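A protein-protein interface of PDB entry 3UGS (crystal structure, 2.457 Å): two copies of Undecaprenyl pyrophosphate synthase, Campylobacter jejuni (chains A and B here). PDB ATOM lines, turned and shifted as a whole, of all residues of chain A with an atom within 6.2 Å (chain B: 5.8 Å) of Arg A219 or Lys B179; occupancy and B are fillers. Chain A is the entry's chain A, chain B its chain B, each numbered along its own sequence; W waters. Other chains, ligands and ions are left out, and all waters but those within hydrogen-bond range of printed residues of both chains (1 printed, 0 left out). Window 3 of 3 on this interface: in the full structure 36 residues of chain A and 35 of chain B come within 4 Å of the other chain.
The backbone NH (N) of Ile A194 is in hydrogen-bond range of the backbone carbonyl oxygen (O) of Lys B179 (2.8 Å). The side-chain carboxylate (OE1) of Glu A193 sits close to the backbone carbonyl oxygen (O) of Lys B179 (3.2 Å). NH1 of Arg B180 is in hydrogen-bond range of O of Glu A220. NH1 of Arg B180 lies within salt-bridge range of OE2 of Glu A193 (2.7 Å).
ND2 of Asn A5 is in hydrogen-bond range of O of Arg A219 (2.6 Å). The side-chain carboxylate (OE2) of Glu B198 is in salt-bridge range of the side-chain amino group (NZ) of Lys B179, 3.7 Å away. NZ of Lys B179 lies within hydrogen-bond range of O of Asn B177 (3.3 Å). O of Arg B180 is in hydrogen-bond range of NH2 of Arg B174 (3.0 Å). OE1 of Glu A193 lies within salt-bridge range of NH2 of Arg A219 (2.5 Å).
Among the printed residues, pairs that only touch across the chains: Ala A192 with Arg B180 (3.2 Å), Phe A196 with Phe B196 (3.3 Å), Arg A219 with Lys B179 (3.5 Å), Ala A192 with Lys B179 (3.9 Å) and Arg A221 with Arg B180 (3.99 Å).
Of chain B, only Lys B179 comes within 4 Å of Arg A219. Lys B179 touches just these residues of chain A: Ala A192 (3.9 Å), Glu A193 (3.2 Å), Ile A194 (2.8 Å) and Arg A219 (3.5 Å). Of the printed residues of chain B, Glu A220 touches Arg B180 (2.9 Å). Of the printed residues of chain B, Ile A194 touches Lys B179 (2.8 Å). Of the printed residues of chain A, Arg B180 touches Ala A192, Glu A193, Glu A220 and Arg A221. The nearest printed residue of chain B that does not touch Arg A219 is Arg B180 (5.9 Å).
Of the 15 printed residues of chain A, 7 touch a printed residue of chain B. Hydrophobic or aromatic side chains of chain A that line the printed part of chain B: Ile A194 and Phe A196. Among the printed residues, Asp or Glu carboxylates within 4 Å of a Lys or Arg side-chain nitrogen of the other chain: Glu A193 with Arg B180 (2.7 Å).
Phe A196 touches its own counterpart, Phe B196. Position printed for both chains: 196.
Water W1 bridges N of Leu B181 (2.5 Å) and O of Ala A192 (2.9 Å).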
ATOM      1  N   ASN A   5      15.816 -12.046  -9.228  1.00  0.00           N
ATOM      2  CA  ASN A   5      16.074 -12.639 -10.559  1.00  0.00           C
ATOM      3  C   ASN A   5      16.632 -11.623 -11.552  1.00  0.00           C
ATOM      4  O   ASN A   5      16.063 -10.552 -11.784  1.00  0.00           O
ATOM      5  CB  ASN A   5      14.815 -13.253 -11.198  1.00  0.00           C
ATOM      6  CG  ASN A   5      14.472 -14.648 -10.664  1.00  0.00           C
ATOM      7  OD1 ASN A   5      15.325 -15.392 -10.141  1.00  0.00           O
ATOM      8  ND2 ASN A   5      13.202 -15.007 -10.796  1.00  0.00           N
ATOM      9  N   LEU A 171      13.479 -14.596 -20.032  1.00  0.00           N
ATOM     10  CA  LEU A 171      12.035 -14.334 -20.287  1.00  0.00           C
ATOM     11  C   LEU A 171      11.735 -14.502 -21.772  1.00  0.00           C
ATOM     12  O   LEU A 171      12.300 -13.832 -22.614  1.00  0.00           O
ATOM     13  CB  LEU A 171      11.603 -12.925 -19.815  1.00  0.00           C
ATOM     14  CG  LEU A 171      10.170 -12.479 -20.157  1.00  0.00           C
ATOM     15  CD1 LEU A 171       9.166 -13.578 -19.791  1.00  0.00           C
ATOM     16  CD2 LEU A 171       9.855 -11.144 -19.451  1.00  0.00           C
ATOM     17  N   ALA A 192      13.663 -21.099 -19.618  1.00  0.00           N
ATOM     18  CA  ALA A 192      13.050 -19.767 -19.814  1.00  0.00           C
ATOM     19  C   ALA A 192      11.674 -19.677 -19.131  1.00  0.00           C
ATOM     20  O   ALA A 192      10.784 -20.538 -19.243  1.00  0.00           O
ATOM     21  CB  ALA A 192      12.929 -19.388 -21.285  1.00  0.00           C
ATOM     22  N   GLU A 193      11.506 -18.583 -18.429  1.00  0.00           N
ATOM     23  CA  GLU A 193      10.167 -18.139 -18.057  1.00  0.00           C
ATOM     24  C   GLU A 193       9.374 -17.755 -19.287  1.00  0.00           C
ATOM     25  O   GLU A 193       9.852 -17.052 -20.162  1.00  0.00           O
ATOM     26  CB  GLU A 193      10.206 -16.987 -17.053  1.00  0.00           C
ATOM     27  CG  GLU A 193      10.781 -17.428 -15.697  1.00  0.00           C
ATOM     28  CD  GLU A 193       9.955 -18.515 -15.019  1.00  0.00           C
ATOM     29  OE1 GLU A 193       8.693 -18.469 -15.126  1.00  0.00           O
ATOM     30  OE2 GLU A 193      10.591 -19.385 -14.358  1.00  0.00           O
ATOM     31  N   ILE A 194       8.163 -18.265 -19.367  1.00  0.00           N
ATOM     32  CA  ILE A 194       7.281 -17.983 -20.514  1.00  0.00           C
ATOM     33  C   ILE A 194       6.115 -17.057 -20.146  1.00  0.00           C
ATOM     34  O   ILE A 194       5.537 -17.155 -19.096  1.00  0.00           O
ATOM     35  CB  ILE A 194       6.709 -19.240 -21.179  1.00  0.00           C
ATOM     36  CG1 ILE A 194       7.818 -20.208 -21.522  1.00  0.00           C
ATOM     37  CG2 ILE A 194       5.953 -18.884 -22.464  1.00  0.00           C
ATOM     38  CD1 ILE A 194       7.260 -21.523 -22.054  1.00  0.00           C
ATOM     39  N   TYR A 195       5.803 -16.148 -21.037  1.00  0.00           N
ATOM     40  CA  TYR A 195       4.750 -15.183 -20.801  1.00  0.00           C
ATOM     41  C   TYR A 195       3.919 -14.895 -22.030  1.00  0.00           C
ATOM     42  O   TYR A 195       4.382 -14.380 -23.025  1.00  0.00           O
ATOM     43  CB  TYR A 195       5.287 -13.880 -20.209  1.00  0.00           C
ATOM     44  CG  TYR A 195       4.164 -13.074 -19.622  1.00  0.00           C
ATOM     45  CD1 TYR A 195       3.826 -13.179 -18.273  1.00  0.00           C
ATOM     46  CD2 TYR A 195       3.355 -12.256 -20.448  1.00  0.00           C
ATOM     47  CE1 TYR A 195       2.739 -12.463 -17.746  1.00  0.00           C
ATOM     48  CE2 TYR A 195       2.273 -11.542 -19.937  1.00  0.00           C
ATOM     49  CZ  TYR A 195       1.971 -11.634 -18.597  1.00  0.00           C
ATOM     50  OH  TYR A 195       0.896 -10.903 -18.148  1.00  0.00           O
ATOM     51  N   PHE A 196       2.655 -15.227 -21.924  1.00  0.00           N
ATOM     52  CA  PHE A 196       1.695 -15.038 -23.028  1.00  0.00           C
ATOM     53  C   PHE A 196       0.876 -13.788 -22.791  1.00  0.00           C
ATOM     54  O   PHE A 196       0.003 -13.763 -21.936  1.00  0.00           O
ATOM     55  CB  PHE A 196       0.767 -16.230 -23.208  1.00  0.00           C
ATOM     56  CG  PHE A 196       1.475 -17.492 -23.602  1.00  0.00           C
ATOM     57  CD1 PHE A 196       2.425 -17.479 -24.583  1.00  0.00           C
ATOM     58  CD2 PHE A 196       1.176 -18.696 -22.992  1.00  0.00           C
ATOM     59  CE1 PHE A 196       3.077 -18.640 -24.962  1.00  0.00           C
ATOM     60  CE2 PHE A 196       1.816 -19.855 -23.373  1.00  0.00           C
ATOM     61  CZ  PHE A 196       2.768 -19.828 -24.362  1.00  0.00           C
ATOM     62  N   LYS A 214       8.833  -6.884 -14.053  1.00  0.00           N
ATOM     63  CA  LYS A 214       8.727  -6.914 -12.559  1.00  0.00           C
ATOM     64  C   LYS A 214       8.267  -8.284 -12.095  1.00  0.00           C
ATOM     65  O   LYS A 214       8.885  -8.938 -11.235  1.00  0.00           O
ATOM     66  CB  LYS A 214       7.727  -5.861 -12.015  1.00  0.00           C
ATOM     67  N   GLU A 215       7.173  -8.697 -12.722  1.00  0.00           N
ATOM     68  CA  GLU A 215       6.572 -10.033 -12.501  1.00  0.00           C
ATOM     69  C   GLU A 215       7.632 -11.123 -12.576  1.00  0.00           C
ATOM     70  O   GLU A 215       7.735 -11.998 -11.713  1.00  0.00           O
ATOM     71  CB  GLU A 215       5.464 -10.337 -13.522  1.00  0.00           C
ATOM     72  CG  GLU A 215       4.773 -11.678 -13.256  1.00  0.00           C
ATOM     73  N   PHE A 216       8.440 -11.017 -13.617  1.00  0.00           N
ATOM     74  CA  PHE A 216       9.499 -11.998 -13.887  1.00  0.00           C
ATOM     75  C   PHE A 216      10.531 -12.061 -12.753  1.00  0.00           C
ATOM     76  O   PHE A 216      10.890 -13.138 -12.228  1.00  0.00           O
ATOM     77  CB  PHE A 216      10.217 -11.725 -15.238  1.00  0.00           C
ATOM     78  CG  PHE A 216      11.553 -12.434 -15.365  1.00  0.00           C
ATOM     79  CD1 PHE A 216      11.607 -13.771 -15.700  1.00  0.00           C
ATOM     80  CD2 PHE A 216      12.725 -11.788 -15.037  1.00  0.00           C
ATOM     81  CE1 PHE A 216      12.816 -14.446 -15.732  1.00  0.00           C
ATOM     82  CE2 PHE A 216      13.935 -12.440 -15.091  1.00  0.00           C
ATOM     83  CZ  PHE A 216      13.981 -13.788 -15.436  1.00  0.00           C
ATOM     84  N   ARG A 217      11.052 -10.890 -12.430  1.00  0.00           N
ATOM     85  CA  ARG A 217      12.120 -10.770 -11.393  1.00  0.00           C
ATOM     86  C   ARG A 217      11.719 -11.430 -10.072  1.00  0.00           C
ATOM     87  O   ARG A 217      12.535 -12.024  -9.370  1.00  0.00           O
ATOM     88  CB  ARG A 217      12.487  -9.318 -11.124  1.00  0.00           C
ATOM     89  CG  ARG A 217      13.041  -8.646 -12.348  1.00  0.00           C
ATOM     90  CD  ARG A 217      13.809  -7.399 -12.008  1.00  0.00           C
ATOM     91  NE  ARG A 217      14.761  -7.080 -13.069  1.00  0.00           N
ATOM     92  CZ  ARG A 217      14.754  -5.953 -13.769  1.00  0.00           C
ATOM     93  NH1 ARG A 217      13.848  -5.011 -13.521  1.00  0.00           N
ATOM     94  NH2 ARG A 217      15.675  -5.748 -14.706  1.00  0.00           N
ATOM     95  N   ASN A 218      10.436 -11.332  -9.767  1.00  0.00           N
ATOM     96  CA  ASN A 218       9.903 -11.886  -8.503  1.00  0.00           C
ATOM     97  C   ASN A 218       9.523 -13.363  -8.501  1.00  0.00           C
ATOM     98  O   ASN A 218       9.618 -14.013  -7.480  1.00  0.00           O
ATOM     99  CB  ASN A 218       8.740 -11.046  -7.984  1.00  0.00           C
ATOM    100  CG  ASN A 218       9.206  -9.739  -7.357  1.00  0.00           C
ATOM    101  OD1 ASN A 218       8.652  -8.686  -7.667  1.00  0.00           O
ATOM    102  ND2 ASN A 218      10.244  -9.790  -6.501  1.00  0.00           N
ATOM    103  N   ARG A 219       9.089 -13.889  -9.632  1.00  0.00           N
ATOM    104  CA  ARG A 219       8.688 -15.304  -9.663  1.00  0.00           C
ATOM    105  C   ARG A 219       9.880 -16.229  -9.504  1.00  0.00           C
ATOM    106  O   ARG A 219      10.982 -15.964  -9.936  1.00  0.00           O
ATOM    107  CB  ARG A 219       7.868 -15.675 -10.871  1.00  0.00           C
ATOM    108  CG  ARG A 219       8.417 -15.165 -12.184  1.00  0.00           C
ATOM    109  CD  ARG A 219       7.930 -16.013 -13.334  1.00  0.00           C
ATOM    110  NE  ARG A 219       6.717 -15.500 -13.951  1.00  0.00           N
ATOM    111  CZ  ARG A 219       6.298 -15.887 -15.150  1.00  0.00           C
ATOM    112  NH1 ARG A 219       5.204 -15.383 -15.694  1.00  0.00           N
ATOM    113  NH2 ARG A 219       6.993 -16.792 -15.814  1.00  0.00           N
ATOM    114  N   GLU A 220       9.607 -17.311  -8.827  1.00  0.00           N
ATOM    115  CA  GLU A 220      10.645 -18.244  -8.400  1.00  0.00           C
ATOM    116  C   GLU A 220      11.189 -19.075  -9.572  1.00  0.00           C
ATOM    117  O   GLU A 220      10.440 -19.706 -10.296  1.00  0.00           O
ATOM    118  CB  GLU A 220      10.136 -19.168  -7.276  1.00  0.00           C
ATOM    119  CG  GLU A 220      11.165 -20.138  -6.699  1.00  0.00           C
ATOM    120  CD  GLU A 220      10.584 -21.033  -5.604  1.00  0.00           C
ATOM    121  OE1 GLU A 220       9.435 -20.782  -5.149  1.00  0.00           O
ATOM    122  OE2 GLU A 220      11.263 -21.991  -5.180  1.00  0.00           O
ATOM    123  N   ARG A 221      12.514 -19.034  -9.705  1.00  0.00           N
ATOM    124  CA  ARG A 221      13.290 -19.868 -10.656  1.00  0.00           C
ATOM    125  C   ARG A 221      14.213 -20.830  -9.927  1.00  0.00           C
ATOM    126  O   ARG A 221      15.157 -20.441  -9.272  1.00  0.00           O
ATOM    127  CB  ARG A 221      14.117 -19.039 -11.636  1.00  0.00           C
ATOM    128  CG  ARG A 221      13.305 -17.996 -12.389  1.00  0.00           C
ATOM    129  CD  ARG A 221      14.191 -17.284 -13.369  1.00  0.00           C
ATOM    130  NE  ARG A 221      14.440 -18.105 -14.537  1.00  0.00           N
ATOM    131  CZ  ARG A 221      15.330 -17.831 -15.482  1.00  0.00           C
ATOM    132  NH1 ARG A 221      16.120 -16.756 -15.411  1.00  0.00           N
ATOM    133  NH2 ARG A 221      15.424 -18.659 -16.507  1.00  0.00           N
ATOM    134  N   ARG B 174       0.753 -27.631 -18.790  1.00  0.00           N
ATOM    135  CA  ARG B 174       1.346 -27.368 -17.471  1.00  0.00           C
ATOM    136  C   ARG B 174       0.213 -27.290 -16.432  1.00  0.00           C
ATOM    137  O   ARG B 174      -0.720 -26.520 -16.567  1.00  0.00           O
ATOM    138  CB  ARG B 174       2.181 -26.082 -17.459  1.00  0.00           C
ATOM    139  CG  ARG B 174       2.389 -25.473 -16.076  1.00  0.00           C
ATOM    140  CD  ARG B 174       3.359 -26.270 -15.180  1.00  0.00           C
ATOM    141  NE  ARG B 174       4.743 -26.245 -15.682  1.00  0.00           N
ATOM    142  CZ  ARG B 174       5.835 -26.501 -14.961  1.00  0.00           C
ATOM    143  NH1 ARG B 174       5.744 -26.849 -13.689  1.00  0.00           N
ATOM    144  NH2 ARG B 174       7.031 -26.429 -15.521  1.00  0.00           N
ATOM    145  N   GLY B 176      -0.134 -26.275 -12.765  1.00  0.00           N
ATOM    146  CA  GLY B 176       0.505 -25.602 -11.655  1.00  0.00           C
ATOM    147  C   GLY B 176       0.568 -24.118 -11.946  1.00  0.00           C
ATOM    148  O   GLY B 176      -0.068 -23.628 -12.875  1.00  0.00           O
ATOM    149  N   ASN B 177       1.338 -23.423 -11.146  1.00  0.00           N
ATOM    150  CA  ASN B 177       1.576 -21.995 -11.381  1.00  0.00           C
ATOM    151  C   ASN B 177       2.868 -21.615 -12.166  1.00  0.00           C
ATOM    152  O   ASN B 177       2.980 -20.511 -12.697  1.00  0.00           O
ATOM    153  CB  ASN B 177       1.514 -21.199 -10.078  1.00  0.00           C
ATOM    154  CG  ASN B 177       1.370 -19.717 -10.339  1.00  0.00           C
ATOM    155  OD1 ASN B 177       0.573 -19.287 -11.209  1.00  0.00           O
ATOM    156  ND2 ASN B 177       2.176 -18.926  -9.647  1.00  0.00           N
ATOM    157  N   ALA B 178       3.805 -22.552 -12.249  1.00  0.00           N
ATOM    158  CA  ALA B 178       5.083 -22.372 -13.015  1.00  0.00           C
ATOM    159  C   ALA B 178       4.802 -22.178 -14.503  1.00  0.00           C
ATOM    160  O   ALA B 178       4.007 -22.884 -15.096  1.00  0.00           O
ATOM    161  CB  ALA B 178       6.029 -23.556 -12.837  1.00  0.00           C
ATOM    162  N   LYS B 179       5.434 -21.181 -15.078  1.00  0.00           N
ATOM    163  CA  LYS B 179       5.287 -20.896 -16.496  1.00  0.00           C
ATOM    164  C   LYS B 179       6.575 -21.118 -17.253  1.00  0.00           C
ATOM    165  O   LYS B 179       7.353 -20.187 -17.459  1.00  0.00           O
ATOM    166  CB  LYS B 179       4.852 -19.467 -16.741  1.00  0.00           C
ATOM    167  CG  LYS B 179       3.646 -19.040 -15.949  1.00  0.00           C
ATOM    168  CD  LYS B 179       2.468 -18.675 -16.842  1.00  0.00           C
ATOM    169  CE  LYS B 179       1.253 -18.327 -16.005  1.00  0.00           C
ATOM    170  NZ  LYS B 179       0.930 -19.454 -15.066  1.00  0.00           N
ATOM    171  N   ARG B 180       6.746 -22.350 -17.718  1.00  0.00           N
ATOM    172  CA  ARG B 180       8.032 -22.801 -18.278  1.00  0.00           C
ATOM    173  C   ARG B 180       8.012 -24.273 -18.634  1.00  0.00           C
ATOM    174  O   ARG B 180       7.126 -24.980 -18.198  1.00  0.00           O
ATOM    175  CB  ARG B 180       9.165 -22.515 -17.318  1.00  0.00           C
ATOM    176  CG  ARG B 180       8.950 -23.160 -15.963  1.00  0.00           C
ATOM    177  CD  ARG B 180      10.091 -22.856 -15.024  1.00  0.00           C
ATOM    178  NE  ARG B 180       9.864 -23.408 -13.694  1.00  0.00           N
ATOM    179  CZ  ARG B 180       9.903 -22.710 -12.561  1.00  0.00           C
ATOM    180  NH1 ARG B 180      10.143 -21.402 -12.573  1.00  0.00           N
ATOM    181  NH2 ARG B 180       9.731 -23.342 -11.411  1.00  0.00           N
ATOM    182  N   LEU B 181       8.961 -24.701 -19.461  1.00  0.00           N
ATOM    183  CA  LEU B 181       8.988 -26.111 -19.946  1.00  0.00           C
ATOM    184  C   LEU B 181       9.926 -27.002 -19.178  1.00  0.00           C
ATOM    185  O   LEU B 181       9.851 -28.206 -19.222  1.00  0.00           O
ATOM    186  CB  LEU B 181       9.316 -26.211 -21.434  1.00  0.00           C
ATOM    187  CG  LEU B 181       8.248 -25.557 -22.364  1.00  0.00           C
ATOM    188  CD1 LEU B 181       8.471 -26.035 -23.790  1.00  0.00           C
ATOM    189  CD2 LEU B 181       6.828 -25.869 -21.932  1.00  0.00           C
ATOM    190  N   PHE B 196      -1.333 -23.426 -19.991  1.00  0.00           N
ATOM    191  CA  PHE B 196      -1.125 -23.316 -18.538  1.00  0.00           C
ATOM    192  C   PHE B 196      -2.452 -23.339 -17.772  1.00  0.00           C
ATOM    193  O   PHE B 196      -3.209 -22.394 -17.827  1.00  0.00           O
ATOM    194  CB  PHE B 196      -0.395 -22.023 -18.163  1.00  0.00           C
ATOM    195  CG  PHE B 196       0.962 -21.885 -18.789  1.00  0.00           C
ATOM    196  CD1 PHE B 196       1.991 -22.790 -18.490  1.00  0.00           C
ATOM    197  CD2 PHE B 196       1.227 -20.842 -19.657  1.00  0.00           C
ATOM    198  CE1 PHE B 196       3.246 -22.658 -19.069  1.00  0.00           C
ATOM    199  CE2 PHE B 196       2.487 -20.706 -20.226  1.00  0.00           C
ATOM    200  CZ  PHE B 196       3.498 -21.616 -19.931  1.00  0.00           C
ATOM    201  N   GLU B 198      -3.957 -23.343 -14.110  1.00  0.00           N
ATOM    202  CA  GLU B 198      -3.490 -22.991 -12.755  1.00  0.00           C
ATOM    203  C   GLU B 198      -4.398 -23.614 -11.689  1.00  0.00           C
ATOM    204  O   GLU B 198      -5.447 -23.107 -11.327  1.00  0.00           O
ATOM    205  CB  GLU B 198      -3.326 -21.500 -12.574  1.00  0.00           C
ATOM    206  CG  GLU B 198      -2.345 -20.914 -13.573  1.00  0.00           C
ATOM    207  CD  GLU B 198      -2.258 -19.396 -13.507  1.00  0.00           C
ATOM    208  OE1 GLU B 198      -2.725 -18.729 -14.464  1.00  0.00           O
ATOM    209  OE2 GLU B 198      -1.728 -18.865 -12.497  1.00  0.00           O
HETATM  210  O   HOH W   1      11.051 -23.336 -19.938  1.00  0.00           O
